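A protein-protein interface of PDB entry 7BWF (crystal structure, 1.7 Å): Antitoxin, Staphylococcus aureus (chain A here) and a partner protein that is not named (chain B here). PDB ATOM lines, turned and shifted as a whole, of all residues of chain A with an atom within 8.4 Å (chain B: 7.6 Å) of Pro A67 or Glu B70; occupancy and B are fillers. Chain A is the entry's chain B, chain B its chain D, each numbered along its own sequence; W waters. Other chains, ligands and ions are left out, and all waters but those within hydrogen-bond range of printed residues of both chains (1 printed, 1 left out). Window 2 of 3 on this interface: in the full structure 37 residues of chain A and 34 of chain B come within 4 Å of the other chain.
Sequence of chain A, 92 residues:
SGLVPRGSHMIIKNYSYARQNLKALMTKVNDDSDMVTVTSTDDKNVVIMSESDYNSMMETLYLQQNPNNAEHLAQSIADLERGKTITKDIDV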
ATOM      1  N   TYR A  62     -19.653  21.968  25.781  1.00  0.00           N
ATOM      2  CA  TYR A  62     -18.425  22.285  26.501  1.00  0.00           C
ATOM      3  C   TYR A  62     -17.402  21.165  26.367  1.00  0.00           C
ATOM      4  O   TYR A  62     -16.211  21.408  26.153  1.00  0.00           O
ATOM      5  CB  TYR A  62     -18.739  22.530  27.971  1.00  0.00           C
ATOM      6  CG  TYR A  62     -17.503  22.734  28.802  1.00  0.00           C
ATOM      7  CD1 TYR A  62     -16.678  23.826  28.587  1.00  0.00           C
ATOM      8  CD2 TYR A  62     -17.164  21.841  29.806  1.00  0.00           C
ATOM      9  CE1 TYR A  62     -15.555  24.022  29.345  1.00  0.00           C
ATOM     10  CE2 TYR A  62     -16.043  22.031  30.572  1.00  0.00           C
ATOM     11  CZ  TYR A  62     -15.237  23.121  30.336  1.00  0.00           C
ATOM     12  OH  TYR A  62     -14.109  23.322  31.094  1.00  0.00           O
ATOM     13  N   LEU A  63     -17.849  19.919  26.495  1.00  0.00           N
ATOM     14  CA  LEU A  63     -16.913  18.802  26.495  1.00  0.00           C
ATOM     15  C   LEU A  63     -16.397  18.506  25.094  1.00  0.00           C
ATOM     16  O   LEU A  63     -15.263  18.040  24.929  1.00  0.00           O
ATOM     17  CB  LEU A  63     -17.585  17.558  27.085  1.00  0.00           C
ATOM     18  CG  LEU A  63     -17.836  17.596  28.591  1.00  0.00           C
ATOM     19  CD1 LEU A  63     -18.792  16.479  29.007  1.00  0.00           C
ATOM     20  CD2 LEU A  63     -16.512  17.488  29.340  1.00  0.00           C
ATOM     21  N   GLN A  64     -17.195  18.788  24.074  1.00  0.00           N
ATOM     22  CA  GLN A  64     -16.831  18.415  22.717  1.00  0.00           C
ATOM     23  C   GLN A  64     -16.089  19.507  21.961  1.00  0.00           C
ATOM     24  O   GLN A  64     -15.551  19.230  20.880  1.00  0.00           O
ATOM     25  CB  GLN A  64     -18.082  18.044  21.914  1.00  0.00           C
ATOM     26  CG  GLN A  64     -18.628  16.648  22.189  1.00  0.00           C
ATOM     27  CD  GLN A  64     -19.818  16.323  21.301  1.00  0.00           C
ATOM     28  OE1 GLN A  64     -20.480  17.225  20.779  1.00  0.00           O
ATOM     29  NE2 GLN A  64     -20.094  15.036  21.125  1.00  0.00           N
ATOM     30  N   GLN A  65     -16.067  20.737  22.478  1.00  0.00           N
ATOM     31  CA  GLN A  65     -15.657  21.866  21.650  1.00  0.00           C
ATOM     32  C   GLN A  65     -14.152  21.909  21.436  1.00  0.00           C
ATOM     33  O   GLN A  65     -13.685  22.587  20.511  1.00  0.00           O
ATOM     34  CB  GLN A  65     -16.165  23.172  22.270  1.00  0.00           C
ATOM     35  CG  GLN A  65     -15.459  23.589  23.544  1.00  0.00           C
ATOM     36  CD  GLN A  65     -16.172  24.731  24.246  1.00  0.00           C
ATOM     37  OE1 GLN A  65     -17.242  25.170  23.816  1.00  0.00           O
ATOM     38  NE2 GLN A  65     -15.579  25.224  25.324  1.00  0.00           N
ATOM     39  N   ASN A  66     -13.387  21.219  22.276  1.00  0.00           N
ATOM     40  CA  ASN A  66     -11.949  21.141  22.118  1.00  0.00           C
ATOM     41  C   ASN A  66     -11.696  19.813  21.438  1.00  0.00           C
ATOM     42  O   ASN A  66     -11.989  18.763  22.044  1.00  0.00           O
ATOM     43  CB  ASN A  66     -11.241  21.178  23.454  1.00  0.00           C
ATOM     44  CG  ASN A  66      -9.724  21.089  23.293  1.00  0.00           C
ATOM     45  OD1 ASN A  66      -9.169  20.047  22.911  1.00  0.00           O
ATOM     46  ND2 ASN A  66      -9.059  22.211  23.503  1.00  0.00           N
ATOM     47  N   PRO A  67     -11.183  19.791  20.207  1.00  0.00           N
ATOM     48  CA  PRO A  67     -11.037  18.493  19.522  1.00  0.00           C
ATOM     49  C   PRO A  67     -10.243  17.480  20.324  1.00  0.00           C
ATOM     50  O   PRO A  67     -10.555  16.286  20.279  1.00  0.00           O
ATOM     51  CB  PRO A  67     -10.321  18.859  18.227  1.00  0.00           C
ATOM     52  CG  PRO A  67     -10.706  20.300  18.016  1.00  0.00           C
ATOM     53  CD  PRO A  67     -10.744  20.928  19.370  1.00  0.00           C
ATOM     54  N   ASN A  68      -9.265  17.935  21.118  1.00  0.00           N
ATOM     55  CA  ASN A  68      -8.427  17.013  21.877  1.00  0.00           C
ATOM     56  C   ASN A  68      -9.210  16.402  23.026  1.00  0.00           C
ATOM     57  O   ASN A  68      -9.090  15.205  23.297  1.00  0.00           O
ATOM     58  CB  ASN A  68      -7.167  17.726  22.396  1.00  0.00           C
ATOM     59  CG  ASN A  68      -6.227  18.139  21.278  1.00  0.00           C
ATOM     60  OD1 ASN A  68      -5.838  17.317  20.448  1.00  0.00           O
ATOM     61  ND2 ASN A  68      -5.887  19.426  21.230  1.00  0.00           N
ATOM     62  N   ASN A  69     -10.031  17.200  23.703  1.00  0.00           N
ATOM     63  CA  ASN A  69     -10.887  16.628  24.732  1.00  0.00           C
ATOM     64  C   ASN A  69     -11.921  15.696  24.116  1.00  0.00           C
ATOM     65  O   ASN A  69     -12.178  14.610  24.644  1.00  0.00           O
ATOM     66  CB  ASN A  69     -11.583  17.719  25.538  1.00  0.00           C
ATOM     67  CG  ASN A  69     -12.163  17.180  26.825  1.00  0.00           C
ATOM     68  OD1 ASN A  69     -11.432  16.805  27.747  1.00  0.00           O
ATOM     69  ND2 ASN A  69     -13.482  17.090  26.878  1.00  0.00           N
ATOM     70  N   ALA A  70     -12.514  16.099  22.990  1.00  0.00           N
ATOM     71  CA  ALA A  70     -13.490  15.243  22.322  1.00  0.00           C
ATOM     72  C   ALA A  70     -12.871  13.900  21.950  1.00  0.00           C
ATOM     73  O   ALA A  70     -13.505  12.852  22.093  1.00  0.00           O
ATOM     74  CB  ALA A  70     -14.044  15.943  21.073  1.00  0.00           C
ATOM     75  N   GLU A  71     -11.627  13.911  21.471  1.00  0.00           N
ATOM     76  CA  GLU A  71     -10.967  12.661  21.102  1.00  0.00           C
ATOM     77  C   GLU A  71     -10.643  11.831  22.340  1.00  0.00           C
ATOM     78  O   GLU A  71     -10.783  10.604  22.329  1.00  0.00           O
ATOM     79  CB  GLU A  71      -9.695  12.962  20.302  1.00  0.00           C
ATOM     80  CG  GLU A  71      -8.874  11.735  19.964  1.00  0.00           C
ATOM     81  CD  GLU A  71      -9.620  10.772  19.062  1.00  0.00           C
ATOM     82  OE1 GLU A  71     -10.603  11.197  18.421  1.00  0.00           O
ATOM     83  OE2 GLU A  71      -9.225   9.592  19.003  1.00  0.00           O
ATOM     84  N   HIS A  72     -10.211  12.485  23.417  1.00  0.00           N
ATOM     85  CA  HIS A  72      -9.972  11.795  24.681  1.00  0.00           C
ATOM     86  C   HIS A  72     -11.245  11.102  25.167  1.00  0.00           C
ATOM     87  O   HIS A  72     -11.213   9.936  25.574  1.00  0.00           O
ATOM     88  CB  HIS A  72      -9.429  12.809  25.701  1.00  0.00           C
ATOM     89  CG  HIS A  72      -9.745  12.487  27.130  1.00  0.00           C
ATOM     90  ND1 HIS A  72      -9.219  11.392  27.785  1.00  0.00           N
ATOM     91  CD2 HIS A  72     -10.514  13.136  28.036  1.00  0.00           C
ATOM     92  CE1 HIS A  72      -9.668  11.371  29.028  1.00  0.00           C
ATOM     93  NE2 HIS A  72     -10.454  12.418  29.205  1.00  0.00           N
ATOM     94  N   LEU A  73     -12.389  11.779  25.065  1.00  0.00           N
ATOM     95  CA  LEU A  73     -13.647  11.185  25.509  1.00  0.00           C
ATOM     96  C   LEU A  73     -14.065  10.037  24.593  1.00  0.00           C
ATOM     97  O   LEU A  73     -14.478   8.971  25.062  1.00  0.00           O
ATOM     98  CB  LEU A  73     -14.741  12.256  25.559  1.00  0.00           C
ATOM     99  CG  LEU A  73     -14.590  13.325  26.641  1.00  0.00           C
ATOM    100  CD1 LEU A  73     -15.763  14.298  26.599  1.00  0.00           C
ATOM    101  CD2 LEU A  73     -14.463  12.685  28.014  1.00  0.00           C
ATOM    102  N   ALA A  74     -13.969  10.236  23.277  1.00  0.00           N
ATOM    103  CA  ALA A  74     -14.380   9.194  22.338  1.00  0.00           C
ATOM    104  C   ALA A  74     -13.520   7.947  22.508  1.00  0.00           C
ATOM    105  O   ALA A  74     -14.031   6.823  22.555  1.00  0.00           O
ATOM    106  CB  ALA A  74     -14.297   9.717  20.898  1.00  0.00           C
ATOM    107  N   LEU B  62     -21.331  20.438  13.733  1.00  0.00           N
ATOM    108  CA  LEU B  62     -20.034  20.624  13.089  1.00  0.00           C
ATOM    109  C   LEU B  62     -18.896  20.195  14.008  1.00  0.00           C
ATOM    110  O   LEU B  62     -17.888  19.645  13.553  1.00  0.00           O
ATOM    111  CB  LEU B  62     -19.869  22.086  12.669  1.00  0.00           C
ATOM    112  CG  LEU B  62     -20.755  22.542  11.510  1.00  0.00           C
ATOM    113  CD1 LEU B  62     -20.813  24.063  11.453  1.00  0.00           C
ATOM    114  CD2 LEU B  62     -20.224  21.960  10.206  1.00  0.00           C
ATOM    115  N   GLN B  63     -19.042  20.421  15.305  1.00  0.00           N
ATOM    116  CA  GLN B  63     -17.960  20.141  16.237  1.00  0.00           C
ATOM    117  C   GLN B  63     -17.947  18.706  16.738  1.00  0.00           C
ATOM    118  O   GLN B  63     -16.951  18.285  17.343  1.00  0.00           O
ATOM    119  CB  GLN B  63     -18.057  21.079  17.446  1.00  0.00           C
ATOM    120  CG  GLN B  63     -17.588  22.503  17.179  1.00  0.00           C
ATOM    121  CD  GLN B  63     -17.625  23.372  18.422  1.00  0.00           C
ATOM    122  OE1 GLN B  63     -16.894  24.351  18.527  1.00  0.00           O
ATOM    123  NE2 GLN B  63     -18.490  23.022  19.368  1.00  0.00           N
ATOM    124  N   ASN B  65     -17.705  15.756  15.534  1.00  0.00           N
ATOM    125  CA  ASN B  65     -16.768  14.782  15.009  1.00  0.00           C
ATOM    126  C   ASN B  65     -15.404  15.395  15.217  1.00  0.00           C
ATOM    127  O   ASN B  65     -15.122  16.451  14.617  1.00  0.00           O
ATOM    128  CB  ASN B  65     -17.000  14.500  13.528  1.00  0.00           C
ATOM    129  CG  ASN B  65     -15.993  13.480  12.974  1.00  0.00           C
ATOM    130  OD1 ASN B  65     -14.799  13.770  12.821  1.00  0.00           O
ATOM    131  ND2 ASN B  65     -16.460  12.260  12.758  1.00  0.00           N
ATOM    132  N   PRO B  66     -14.543  14.813  16.055  1.00  0.00           N
ATOM    133  CA  PRO B  66     -13.259  15.482  16.340  1.00  0.00           C
ATOM    134  C   PRO B  66     -12.471  15.827  15.088  1.00  0.00           C
ATOM    135  O   PRO B  66     -11.802  16.865  15.051  1.00  0.00           O
ATOM    136  CB  PRO B  66     -12.518  14.462  17.203  1.00  0.00           C
ATOM    137  CG  PRO B  66     -13.654  13.682  17.833  1.00  0.00           C
ATOM    138  CD  PRO B  66     -14.669  13.518  16.759  1.00  0.00           C
ATOM    139  N   ASN B  67     -12.606  15.031  14.022  1.00  0.00           N
ATOM    140  CA  ASN B  67     -11.830  15.278  12.811  1.00  0.00           C
ATOM    141  C   ASN B  67     -12.389  16.474  12.060  1.00  0.00           C
ATOM    142  O   ASN B  67     -11.634  17.323  11.582  1.00  0.00           O
ATOM    143  CB  ASN B  67     -11.802  14.030  11.915  1.00  0.00           C
ATOM    144  CG  ASN B  67     -11.043  12.878  12.541  1.00  0.00           C
ATOM    145  OD1 ASN B  67     -11.580  11.783  12.718  1.00  0.00           O
ATOM    146  ND2 ASN B  67      -9.796  13.131  12.913  1.00  0.00           N
ATOM    147  N   ASN B  68     -13.714  16.579  11.976  1.00  0.00           N
ATOM    148  CA  ASN B  68     -14.297  17.772  11.377  1.00  0.00           C
ATOM    149  C   ASN B  68     -13.989  18.999  12.224  1.00  0.00           C
ATOM    150  O   ASN B  68     -13.667  20.068  11.690  1.00  0.00           O
ATOM    151  CB  ASN B  68     -15.804  17.621  11.205  1.00  0.00           C
ATOM    152  CG  ASN B  68     -16.367  18.643  10.239  1.00  0.00           C
ATOM    153  OD1 ASN B  68     -16.131  18.568   9.028  1.00  0.00           O
ATOM    154  ND2 ASN B  68     -17.074  19.629  10.770  1.00  0.00           N
ATOM    155  N   ALA B  69     -14.059  18.860  13.549  1.00  0.00           N
ATOM    156  CA  ALA B  69     -13.748  19.985  14.425  1.00  0.00           C
ATOM    157  C   ALA B  69     -12.321  20.473  14.190  1.00  0.00           C
ATOM    158  O   ALA B  69     -12.069  21.680  14.140  1.00  0.00           O
ATOM    159  CB  ALA B  69     -13.961  19.591  15.894  1.00  0.00           C
ATOM    160  N   GLU B  70     -11.374  19.549  14.021  1.00  0.00           N
ATOM    161  CA  GLU B  70      -9.992  19.955  13.783  1.00  0.00           C
ATOM    162  C   GLU B  70      -9.838  20.563  12.392  1.00  0.00           C
ATOM    163  O   GLU B  70      -9.077  21.517  12.200  1.00  0.00           O
ATOM    164  CB  GLU B  70      -9.059  18.755  13.966  1.00  0.00           C
ATOM    165  CG  GLU B  70      -7.610  19.047  13.614  1.00  0.00           C
ATOM    166  CD  GLU B  70      -6.909  19.890  14.664  1.00  0.00           C
ATOM    167  OE1 GLU B  70      -7.371  19.918  15.826  1.00  0.00           O
ATOM    168  OE2 GLU B  70      -5.898  20.533  14.318  1.00  0.00           O
ATOM    169  N   HIS B  71     -10.559  20.029  11.409  1.00  0.00           N
ATOM    170  CA  HIS B  71     -10.514  20.589  10.062  1.00  0.00           C
ATOM    171  C   HIS B  71     -11.046  22.027  10.052  1.00  0.00           C
ATOM    172  O   HIS B  71     -10.457  22.912   9.423  1.00  0.00           O
ATOM    173  CB  HIS B  71     -11.283  19.650   9.113  1.00  0.00           C
ATOM    174  CG  HIS B  71     -12.007  20.352   8.011  1.00  0.00           C
ATOM    175  ND1 HIS B  71     -11.350  20.968   6.966  1.00  0.00           N
ATOM    176  CD2 HIS B  71     -13.332  20.516   7.777  1.00  0.00           C
ATOM    177  CE1 HIS B  71     -12.240  21.506   6.150  1.00  0.00           C
ATOM    178  NE2 HIS B  71     -13.448  21.242   6.617  1.00  0.00           N
ATOM    179  N   LEU B  72     -12.118  22.293  10.801  1.00  0.00           N
ATOM    180  CA  LEU B  72     -12.634  23.657  10.917  1.00  0.00           C
ATOM    181  C   LEU B  72     -11.660  24.560  11.670  1.00  0.00           C
ATOM    182  O   LEU B  72     -11.404  25.694  11.248  1.00  0.00           O
ATOM    183  CB  LEU B  72     -13.994  23.641  11.622  1.00  0.00           C
ATOM    184  CG  LEU B  72     -15.126  23.011  10.810  1.00  0.00           C
ATOM    185  CD1 LEU B  72     -16.422  22.986  11.616  1.00  0.00           C
ATOM    186  CD2 LEU B  72     -15.316  23.746   9.492  1.00  0.00           C
ATOM    187  N   ALA B  73     -11.114  24.085  12.796  1.00  0.00           N
ATOM    188  CA  ALA B  73     -10.188  24.906  13.574  1.00  0.00           C
ATOM    189  C   ALA B  73      -8.969  25.284  12.740  1.00  0.00           C
ATOM    190  O   ALA B  73      -8.585  26.457  12.670  1.00  0.00           O
ATOM    191  CB  ALA B  73      -9.756  24.170  14.849  1.00  0.00           C
ATOM    192  N   GLN B  74      -8.337  24.297  12.105  1.00  0.00           N
ATOM    193  CA  GLN B  74      -7.144  24.585  11.315  1.00  0.00           C
ATOM    194  C   GLN B  74      -7.471  25.546  10.179  1.00  0.00           C
ATOM    195  O   GLN B  74      -6.695  26.463   9.885  1.00  0.00           O
ATOM    196  CB  GLN B  74      -6.543  23.288  10.760  1.00  0.00           C
ATOM    197  CG  GLN B  74      -5.394  23.528   9.795  1.00  0.00           C
ATOM    198  CD  GLN B  74      -4.115  23.935  10.508  1.00  0.00           C
ATOM    199  OE1 GLN B  74      -3.675  23.277  11.453  1.00  0.00           O
ATOM    200  NE2 GLN B  74      -3.526  25.042  10.068  1.00  0.00           N
ATOM    201  N   SER B  75      -8.615  25.348   9.520  1.00  0.00           N
ATOM    202  CA  SER B  75      -8.944  26.159   8.350  1.00  0.00           C
ATOM    203  C   SER B  75      -9.231  27.602   8.747  1.00  0.00           C
ATOM    204  O   SER B  75      -8.842  28.534   8.039  1.00  0.00           O
ATOM    205  CB  SER B  75     -10.140  25.554   7.605  1.00  0.00           C
ATOM    206  OG  SER B  75      -9.817  24.277   7.084  1.00  0.00           O
ATOM    207  N   ILE B  76      -9.903  27.812   9.880  1.00  0.00           N
ATOM    208  CA  ILE B  76     -10.146  29.176  10.340  1.00  0.00           C
ATOM    209  C   ILE B  76      -8.842  29.812  10.814  1.00  0.00           C
ATOM    210  O   ILE B  76      -8.628  31.019  10.640  1.00  0.00           O
ATOM    211  CB  ILE B  76     -11.226  29.193  11.439  1.00  0.00           C
ATOM    212  CG1 ILE B  76     -12.571  28.766  10.849  1.00  0.00           C
ATOM    213  CG2 ILE B  76     -11.318  30.586  12.046  1.00  0.00           C
ATOM    214  CD1 ILE B  76     -13.693  28.628  11.872  1.00  0.00           C
HETATM  215  O   HOH W   1     -18.946  24.216  21.643  1.00  0.00           O
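Gln A64 touches Gln B63 (O to O, 3.9 Å).
Gln A65 touches Gln B63.
Pro A67 touches Ala B69 (CG to CB, 3.9 Å).
Pro A67 touches Glu B70 (CB to OE1, 3.9 Å).
Ala A70 touches Pro B66.
CB of Pro B66 touches OE1 of Glu A71, 3.98 Å away.
Printed residues of chain B within 4 Å of Gln A64: Gln B63 (3.9 Å).
Of the printed residues of chain B, Gln A65 touches Gln B63 (3.7 Å).
Of chain B, only Ala B69 (3.9 Å) and Glu B70 (3.9 Å) come within 4 Å of Pro A67.
Of the printed residues of chain B, Ala A70 touches Pro B66 (3.97 Å).
Of the printed residues of chain B, Glu A71 touches Pro B66 (3.98 Å).
Of the printed residues of chain A, Gln B63 touches Gln A64 and Gln A65.
Glu B70 touches one residue of chain A.
The nearest residue of chain B that does not touch Pro A67 is Pro B66 (4.03 Å).
The nearest residue of chain A that does not touch Glu B70 is Asn A68 (5.5 Å).
Water W1 lies within hydrogen-bond range of the side-chain amide nitrogen (NE2) of Gln B63 (2.6 Å) and the side-chain amide oxygen (OE1) of Gln A65 (2.9 Å).
Printed residues of chain B that touch a printed residue of chain A: Gln B63, Pro B66, Ala B69 and Glu B70.
Hydrophobic or aromatic side chains of chain B that line the printed part of chain A: Pro B66 and Ala B69.
Of the 13 printed residues of chain A, 5 touch a printed residue of chain B.
Hydrophobic or aromatic side chains of chain A that line the printed part of chain B: Pro A67 and Ala A70.
Along chain A the printed residues that touch a printed residue of chain B span positions 64 to 71.
Among the printed residues, 6 pairs touch across the chains.
Among the printed residues, no Asp or Glu carboxylate lies within 4 Å of a Lys or Arg side-chain nitrogen of the other chain.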
